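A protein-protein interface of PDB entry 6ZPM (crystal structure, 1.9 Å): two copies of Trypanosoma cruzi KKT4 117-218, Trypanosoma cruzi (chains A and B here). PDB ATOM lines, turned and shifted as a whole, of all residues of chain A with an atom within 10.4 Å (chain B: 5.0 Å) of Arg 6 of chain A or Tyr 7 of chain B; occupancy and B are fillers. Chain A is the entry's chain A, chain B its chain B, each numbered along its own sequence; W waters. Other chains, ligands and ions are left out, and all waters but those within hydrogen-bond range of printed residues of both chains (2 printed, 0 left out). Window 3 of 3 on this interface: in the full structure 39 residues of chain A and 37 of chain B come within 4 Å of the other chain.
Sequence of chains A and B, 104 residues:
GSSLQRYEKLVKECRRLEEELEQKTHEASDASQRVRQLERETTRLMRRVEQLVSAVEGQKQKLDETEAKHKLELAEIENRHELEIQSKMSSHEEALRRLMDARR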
ATOM      1  N   SER A   2      14.519  -9.134   2.779  1.00  0.00           N
ATOM      2  CA  SER A   2      13.166  -9.729   2.837  1.00  0.00           C
ATOM      3  C   SER A   2      13.322 -11.182   2.450  1.00  0.00           C
ATOM      4  O   SER A   2      12.863 -11.987   3.145  1.00  0.00           O
ATOM      5  CB  SER A   2      12.208  -9.053   1.925  1.00  0.00           C
ATOM      6  N   SER A   3      13.970 -11.435   1.331  1.00  0.00           N
ATOM      7  CA  SER A   3      14.307 -12.816   0.947  1.00  0.00           C
ATOM      8  C   SER A   3      15.043 -13.451   2.136  1.00  0.00           C
ATOM      9  O   SER A   3      14.705 -14.560   2.504  1.00  0.00           O
ATOM     10  CB  SER A   3      15.156 -12.821  -0.277  1.00  0.00           C
ATOM     11  OG  SER A   3      14.367 -12.990  -1.439  1.00  0.00           O
ATOM     12  N   LEU A   4      16.087 -12.825   2.653  1.00  0.00           N
ATOM     13  CA  LEU A   4      16.812 -13.432   3.779  1.00  0.00           C
ATOM     14  C   LEU A   4      15.879 -13.608   4.979  1.00  0.00           C
ATOM     15  O   LEU A   4      15.873 -14.668   5.552  1.00  0.00           O
ATOM     16  CB  LEU A   4      18.023 -12.576   4.112  1.00  0.00           C
ATOM     17  CG  LEU A   4      18.854 -13.077   5.278  1.00  0.00           C
ATOM     18  CD1 LEU A   4      19.286 -14.504   5.085  1.00  0.00           C
ATOM     19  CD2 LEU A   4      20.061 -12.203   5.468  1.00  0.00           C
ATOM     20  N   GLN A   5      15.107 -12.584   5.305  1.00  0.00           N
ATOM     21  CA  GLN A   5      14.238 -12.663   6.476  1.00  0.00           C
ATOM     22  C   GLN A   5      13.170 -13.736   6.304  1.00  0.00           C
ATOM     23  O   GLN A   5      12.818 -14.425   7.267  1.00  0.00           O
ATOM     24  CB  GLN A   5      13.594 -11.302   6.745  1.00  0.00           C
ATOM     25  N   ARG A   6      12.638 -13.892   5.089  1.00  0.00           N
ATOM     26  CA  ARG A   6      11.636 -14.929   4.858  1.00  0.00           C
ATOM     27  C   ARG A   6      12.211 -16.315   5.124  1.00  0.00           C
ATOM     28  O   ARG A   6      11.577 -17.144   5.789  1.00  0.00           O
ATOM     29  CB  ARG A   6      11.102 -14.830   3.429  1.00  0.00           C
ATOM     30  N   TYR A   7      13.425 -16.574   4.633  1.00  0.00           N
ATOM     31  CA  TYR A   7      14.063 -17.869   4.847  1.00  0.00           C
ATOM     32  C   TYR A   7      14.373 -18.103   6.319  1.00  0.00           C
ATOM     33  O   TYR A   7      14.139 -19.201   6.838  1.00  0.00           O
ATOM     34  CB  TYR A   7      15.340 -17.963   4.006  1.00  0.00           C
ATOM     35  CG  TYR A   7      15.911 -19.356   3.906  1.00  0.00           C
ATOM     36  CD1 TYR A   7      16.799 -19.833   4.860  1.00  0.00           C
ATOM     37  CD2 TYR A   7      15.575 -20.193   2.848  1.00  0.00           C
ATOM     38  CE1 TYR A   7      17.326 -21.104   4.774  1.00  0.00           C
ATOM     39  CE2 TYR A   7      16.100 -21.471   2.754  1.00  0.00           C
ATOM     40  CZ  TYR A   7      16.974 -21.922   3.721  1.00  0.00           C
ATOM     41  OH  TYR A   7      17.496 -23.191   3.647  1.00  0.00           O
ATOM     42  N   GLU A   8      14.896 -17.083   7.009  1.00  0.00           N
ATOM     43  CA  GLU A   8      15.271 -17.241   8.413  1.00  0.00           C
ATOM     44  C   GLU A   8      14.054 -17.498   9.297  1.00  0.00           C
ATOM     45  O   GLU A   8      14.147 -18.250  10.276  1.00  0.00           O
ATOM     46  CB  GLU A   8      16.036 -16.002   8.894  1.00  0.00           C
ATOM     47  CG  GLU A   8      17.535 -16.025   8.581  1.00  0.00           C
ATOM     48  CD  GLU A   8      18.234 -14.689   8.843  1.00  0.00           C
ATOM     49  OE1 GLU A   8      17.553 -13.709   9.222  1.00  0.00           O
ATOM     50  OE2 GLU A   8      19.470 -14.619   8.665  1.00  0.00           O
ATOM     51  N   LYS A   9      12.912 -16.895   8.969  1.00  0.00           N
ATOM     52  CA  LYS A   9      11.695 -17.168   9.728  1.00  0.00           C
ATOM     53  C   LYS A   9      11.242 -18.609   9.537  1.00  0.00           C
ATOM     54  O   LYS A   9      10.819 -19.269  10.493  1.00  0.00           O
ATOM     55  CB  LYS A   9      10.589 -16.201   9.311  1.00  0.00           C
ATOM     56  N   LEU A  10      11.318 -19.112   8.305  1.00  0.00           N
ATOM     57  CA  LEU A  10      10.988 -20.509   8.054  1.00  0.00           C
ATOM     58  C   LEU A  10      11.997 -21.451   8.706  1.00  0.00           C
ATOM     59  O   LEU A  10      11.628 -22.550   9.139  1.00  0.00           O
ATOM     60  CB  LEU A  10      10.911 -20.746   6.548  1.00  0.00           C
ATOM     61  CG  LEU A  10      10.456 -22.115   6.050  1.00  0.00           C
ATOM     62  CD1 LEU A  10       9.058 -22.445   6.536  1.00  0.00           C
ATOM     63  CD2 LEU A  10      10.517 -22.117   4.539  1.00  0.00           C
ATOM     64  N   VAL A  11      13.263 -21.032   8.804  1.00  0.00           N
ATOM     65  CA  VAL A  11      14.285 -21.850   9.458  1.00  0.00           C
ATOM     66  C   VAL A  11      13.944 -22.067  10.927  1.00  0.00           C
ATOM     67  O   VAL A  11      14.115 -23.168  11.466  1.00  0.00           O
ATOM     68  CB  VAL A  11      15.669 -21.194   9.292  1.00  0.00           C
ATOM     69  CG1 VAL A  11      16.609 -21.615  10.407  1.00  0.00           C
ATOM     70  CG2 VAL A  11      16.261 -21.533   7.946  1.00  0.00           C
ATOM     71  N   LYS A  12      13.469 -21.019  11.605  1.00  0.00           N
ATOM     72  CA  LYS A  12      13.136 -21.152  13.020  1.00  0.00           C
ATOM     73  C   LYS A  12      11.965 -22.105  13.219  1.00  0.00           C
ATOM     74  O   LYS A  12      11.949 -22.891  14.172  1.00  0.00           O
ATOM     75  CB  LYS A  12      12.826 -19.781  13.618  1.00  0.00           C
ATOM     76  N   GLU A  13      10.973 -22.046  12.326  1.00  0.00           N
ATOM     77  CA  GLU A  13       9.882 -23.010  12.378  1.00  0.00           C
ATOM     78  C   GLU A  13      10.386 -24.425  12.134  1.00  0.00           C
ATOM     79  O   GLU A  13       9.872 -25.381  12.726  1.00  0.00           O
ATOM     80  CB  GLU A  13       8.805 -22.638  11.357  1.00  0.00           C
ATOM     81  CG  GLU A  13       7.679 -23.651  11.230  1.00  0.00           C
ATOM     82  CD  GLU A  13       6.756 -23.649  12.436  1.00  0.00           C
ATOM     83  OE1 GLU A  13       6.855 -22.720  13.263  1.00  0.00           O
ATOM     84  OE2 GLU A  13       5.928 -24.577  12.552  1.00  0.00           O
ATOM     85  N   CYS A  14      11.408 -24.582  11.291  1.00  0.00           N
ATOM     86  CA  CYS A  14      11.895 -25.927  11.011  1.00  0.00           C
ATOM     87  C   CYS A  14      12.588 -26.516  12.246  1.00  0.00           C
ATOM     88  O   CYS A  14      12.440 -27.712  12.527  1.00  0.00           O
ATOM     89  CB  CYS A  14      12.803 -25.892   9.775  1.00  0.00           C
ATOM     90  SG  CYS A  14      13.402 -27.491   9.180  1.00  0.00           S
ATOM     91  N   SER B   2      17.303 -20.964  -8.105  1.00  0.00           N
ATOM     92  CA  SER B   2      18.152 -20.650  -6.962  1.00  0.00           C
ATOM     93  C   SER B   2      17.321 -20.294  -5.727  1.00  0.00           C
ATOM     94  O   SER B   2      16.911 -21.179  -4.983  1.00  0.00           O
ATOM     95  CB  SER B   2      19.101 -19.511  -7.306  1.00  0.00           C
ATOM     96  OG  SER B   2      18.378 -18.317  -7.547  1.00  0.00           O
ATOM     97  N   SER B   3      17.058 -18.998  -5.531  1.00  0.00           N
ATOM     98  CA  SER B   3      16.480 -18.533  -4.270  1.00  0.00           C
ATOM     99  C   SER B   3      15.099 -19.130  -4.026  1.00  0.00           C
ATOM    100  O   SER B   3      14.787 -19.568  -2.910  1.00  0.00           O
ATOM    101  CB  SER B   3      16.402 -17.010  -4.257  1.00  0.00           C
ATOM    102  OG  SER B   3      15.656 -16.573  -3.133  1.00  0.00           O
ATOM    103  N   LEU B   4      14.243 -19.121  -5.048  1.00  0.00           N
ATOM    104  CA  LEU B   4      12.944 -19.764  -4.915  1.00  0.00           C
ATOM    105  C   LEU B   4      13.105 -21.248  -4.618  1.00  0.00           C
ATOM    106  O   LEU B   4      12.413 -21.795  -3.751  1.00  0.00           O
ATOM    107  CB  LEU B   4      12.123 -19.551  -6.185  1.00  0.00           C
ATOM    108  CG  LEU B   4      10.803 -20.314  -6.291  1.00  0.00           C
ATOM    109  CD1 LEU B   4       9.818 -19.797  -5.256  1.00  0.00           C
ATOM    110  CD2 LEU B   4      10.224 -20.199  -7.699  1.00  0.00           C
ATOM    111  N   GLN B   5      14.035 -21.913  -5.310  1.00  0.00           N
ATOM    112  CA  GLN B   5      14.213 -23.344  -5.089  1.00  0.00           C
ATOM    113  C   GLN B   5      14.699 -23.629  -3.674  1.00  0.00           C
ATOM    114  O   GLN B   5      14.250 -24.591  -3.041  1.00  0.00           O
ATOM    115  CB  GLN B   5      15.179 -23.936  -6.116  1.00  0.00           C
ATOM    116  CG  GLN B   5      15.445 -25.425  -5.894  1.00  0.00           C
ATOM    117  CD  GLN B   5      15.972 -26.132  -7.130  1.00  0.00           C
ATOM    118  OE1 GLN B   5      16.669 -25.539  -7.954  1.00  0.00           O
ATOM    119  NE2 GLN B   5      15.640 -27.412  -7.260  1.00  0.00           N
ATOM    120  N   ARG B   6      15.611 -22.799  -3.153  1.00  0.00           N
ATOM    121  CA  ARG B   6      16.105 -23.023  -1.798  1.00  0.00           C
ATOM    122  C   ARG B   6      14.977 -22.906  -0.781  1.00  0.00           C
ATOM    123  O   ARG B   6      14.873 -23.725   0.141  1.00  0.00           O
ATOM    124  CB  ARG B   6      17.231 -22.037  -1.478  1.00  0.00           C
ATOM    125  CG  ARG B   6      18.459 -22.178  -2.373  1.00  0.00           C
ATOM    126  CD  ARG B   6      19.666 -21.406  -1.831  1.00  0.00           C
ATOM    127  NE  ARG B   6      19.376 -19.987  -1.622  1.00  0.00           N
ATOM    128  CZ  ARG B   6      19.492 -19.046  -2.559  1.00  0.00           C
ATOM    129  NH1 ARG B   6      19.894 -19.363  -3.783  1.00  0.00           N
ATOM    130  NH2 ARG B   6      19.209 -17.782  -2.274  1.00  0.00           N
ATOM    131  N   TYR B   7      14.113 -21.903  -0.945  1.00  0.00           N
ATOM    132  CA  TYR B   7      12.991 -21.711  -0.032  1.00  0.00           C
ATOM    133  C   TYR B   7      11.993 -22.862  -0.125  1.00  0.00           C
ATOM    134  O   TYR B   7      11.541 -23.388   0.899  1.00  0.00           O
ATOM    135  CB  TYR B   7      12.310 -20.369  -0.327  1.00  0.00           C
ATOM    136  CG  TYR B   7      11.192 -20.015   0.631  1.00  0.00           C
ATOM    137  CD1 TYR B   7      11.454 -19.358   1.831  1.00  0.00           C
ATOM    138  CD2 TYR B   7       9.874 -20.337   0.337  1.00  0.00           C
ATOM    139  CE1 TYR B   7      10.427 -19.035   2.710  1.00  0.00           C
ATOM    140  CE2 TYR B   7       8.843 -20.019   1.209  1.00  0.00           C
ATOM    141  CZ  TYR B   7       9.124 -19.372   2.391  1.00  0.00           C
ATOM    142  OH  TYR B   7       8.091 -19.065   3.253  1.00  0.00           O
ATOM    143  N   GLU B   8      11.623 -23.271  -1.342  1.00  0.00           N
ATOM    144  CA  GLU B   8      10.654 -24.357  -1.441  1.00  0.00           C
ATOM    145  C   GLU B   8      11.212 -25.659  -0.876  1.00  0.00           C
ATOM    146  O   GLU B   8      10.456 -26.462  -0.319  1.00  0.00           O
ATOM    147  CB  GLU B   8      10.177 -24.527  -2.884  1.00  0.00           C
ATOM    148  CG  GLU B   8      11.226 -24.877  -3.902  1.00  0.00           C
ATOM    149  CD  GLU B   8      10.663 -24.880  -5.317  1.00  0.00           C
ATOM    150  OE1 GLU B   8      10.239 -25.956  -5.787  1.00  0.00           O
ATOM    151  OE2 GLU B   8      10.630 -23.807  -5.955  1.00  0.00           O
ATOM    152  N   LYS B   9      12.529 -25.860  -0.952  1.00  0.00           N
ATOM    153  CA  LYS B   9      13.122 -27.048  -0.343  1.00  0.00           C
ATOM    154  C   LYS B   9      12.966 -27.033   1.174  1.00  0.00           C
ATOM    155  O   LYS B   9      12.740 -28.080   1.792  1.00  0.00           O
ATOM    156  CB  LYS B   9      14.594 -27.151  -0.736  1.00  0.00           C
ATOM    157  CG  LYS B   9      14.796 -27.781  -2.103  1.00  0.00           C
ATOM    158  CD  LYS B   9      16.264 -27.992  -2.406  1.00  0.00           C
ATOM    159  CE  LYS B   9      16.635 -29.454  -2.256  1.00  0.00           C
ATOM    160  NZ  LYS B   9      16.654 -29.862  -0.822  1.00  0.00           N
ATOM    161  N   LEU B  10      13.084 -25.858   1.794  1.00  0.00           N
ATOM    162  CA  LEU B  10      12.878 -25.771   3.235  1.00  0.00           C
ATOM    163  C   LEU B  10      11.404 -25.910   3.592  1.00  0.00           C
ATOM    164  O   LEU B  10      11.068 -26.505   4.624  1.00  0.00           O
ATOM    165  CB  LEU B  10      13.440 -24.452   3.767  1.00  0.00           C
ATOM    166  CG  LEU B  10      13.382 -24.207   5.277  1.00  0.00           C
ATOM    167  CD1 LEU B  10      14.025 -25.324   6.045  1.00  0.00           C
ATOM    168  CD2 LEU B  10      14.042 -22.880   5.592  1.00  0.00           C
ATOM    169  N   VAL B  11      10.511 -25.352   2.767  1.00  0.00           N
ATOM    170  CA  VAL B  11       9.081 -25.568   2.977  1.00  0.00           C
ATOM    171  C   VAL B  11       8.769 -27.056   2.943  1.00  0.00           C
ATOM    172  O   VAL B  11       8.002 -27.567   3.771  1.00  0.00           O
ATOM    173  CB  VAL B  11       8.244 -24.804   1.928  1.00  0.00           C
ATOM    174  CG1 VAL B  11       6.774 -25.224   2.009  1.00  0.00           C
ATOM    175  CG2 VAL B  11       8.365 -23.304   2.111  1.00  0.00           C
HETATM  176  O   HOH W   1       8.710 -17.359   5.319  1.00  0.00           O
HETATM  177  O   HOH W   2      16.994 -24.495   1.475  1.00  0.00           O
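Arg 6 of chain A touches one residue of chain B. Tyr 7 of chain B touches just these residues of chain A: Arg 6 and Leu 10. No residue of chain A comes within 4 Å of Ser 3 of chain B. Of chain A, only Tyr 7 (3.6 Å), Leu 10 (3.6 Å), Val 11 (3.5 Å) and Cys 14 (3.9 Å) come within 4 Å of Leu 10 of chain B. Of chain A, only Leu 10 (3.5 Å) comes within 4 Å of Val 11 of chain B. Of the printed residues of chain B, Val 11 of chain A touches Leu 10 (3.5 Å). Of the printed residues of chain B, Leu 10 of chain A touches Tyr 7 (3.6 Å), Leu 10 (3.6 Å) and Val 11 (3.5 Å). Of the printed residues of chain A, Arg 6 of chain B touches Tyr 7 (3.7 Å). Of the printed residues of chain B, Tyr 7 of chain A touches Arg 6 (3.7 Å) and Leu 10 (3.6 Å). Printed residues of chain B within 4 Å of Cys 14 of chain A: Leu 10 (3.9 Å). Glu 8 of chain A touches none of the printed residues of chain B. Leu 4 of chain B touches none of the printed residues of chain A. The nearest printed residue of chain B that does not touch Arg 6 of chain A is Leu 10 of chain B (6.2 Å). The nearest residue of chain A that does not touch Tyr 7 of chain B is Tyr 7 of chain A (4.2 Å). The nearest printed residue of chain B that does not touch Cys 14 of chain A is Val 11 of chain B (7.4 Å).
Water W2 bridges the side-chain hydroxyl (OH) of Tyr 7 of chain A (2.6 Å) and the backbone carbonyl oxygen (O) of Arg 6 of chain B (2.6 Å). Water W1 bridges the side-chain hydroxyl (OH) of Tyr 7 of chain B (2.7 Å) and the backbone carbonyl oxygen (O) of Arg 6 of chain A (2.9 Å).
Arg 6 of chain A touches Tyr 7 of chain B, and with the chains exchanged Tyr 7 of chain A touches Arg 6 of chain B. Tyr 7 of chain A touches Leu 10 of chain B, and with the chains exchanged Leu 10 of chain A touches Tyr 7 of chain B. Leu 10 of chain A touches its own counterpart, Leu 10 of chain B. Leu 10 of chain A touches Val 11 of chain B, and with the chains exchanged Val 11 of chain A touches Leu 10 of chain B. Of the 8 pairs that touch across the chains among the printed residues, 7 have their exchanged pair printed and touching as well.
Arg 6 of chain A touches Tyr 7 of chain B (O to CE1, 3.8 Å). Arg 6 of chain B touches Tyr 7 of chain A (O to CE2, 3.7 Å). Tyr 7 of chain A touches Leu 10 of chain B. Leu 10 of chain A touches Tyr 7 of chain B. Leu 10 of chain A touches Leu 10 of chain B (CD2 to CG, 3.6 Å). Leu 10 of chain A touches Val 11 of chain B. Val 11 of chain A touches Leu 10 of chain B (CG2 to CD2, 3.5 Å). Cys 14 of chain A touches Leu 10 of chain B.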
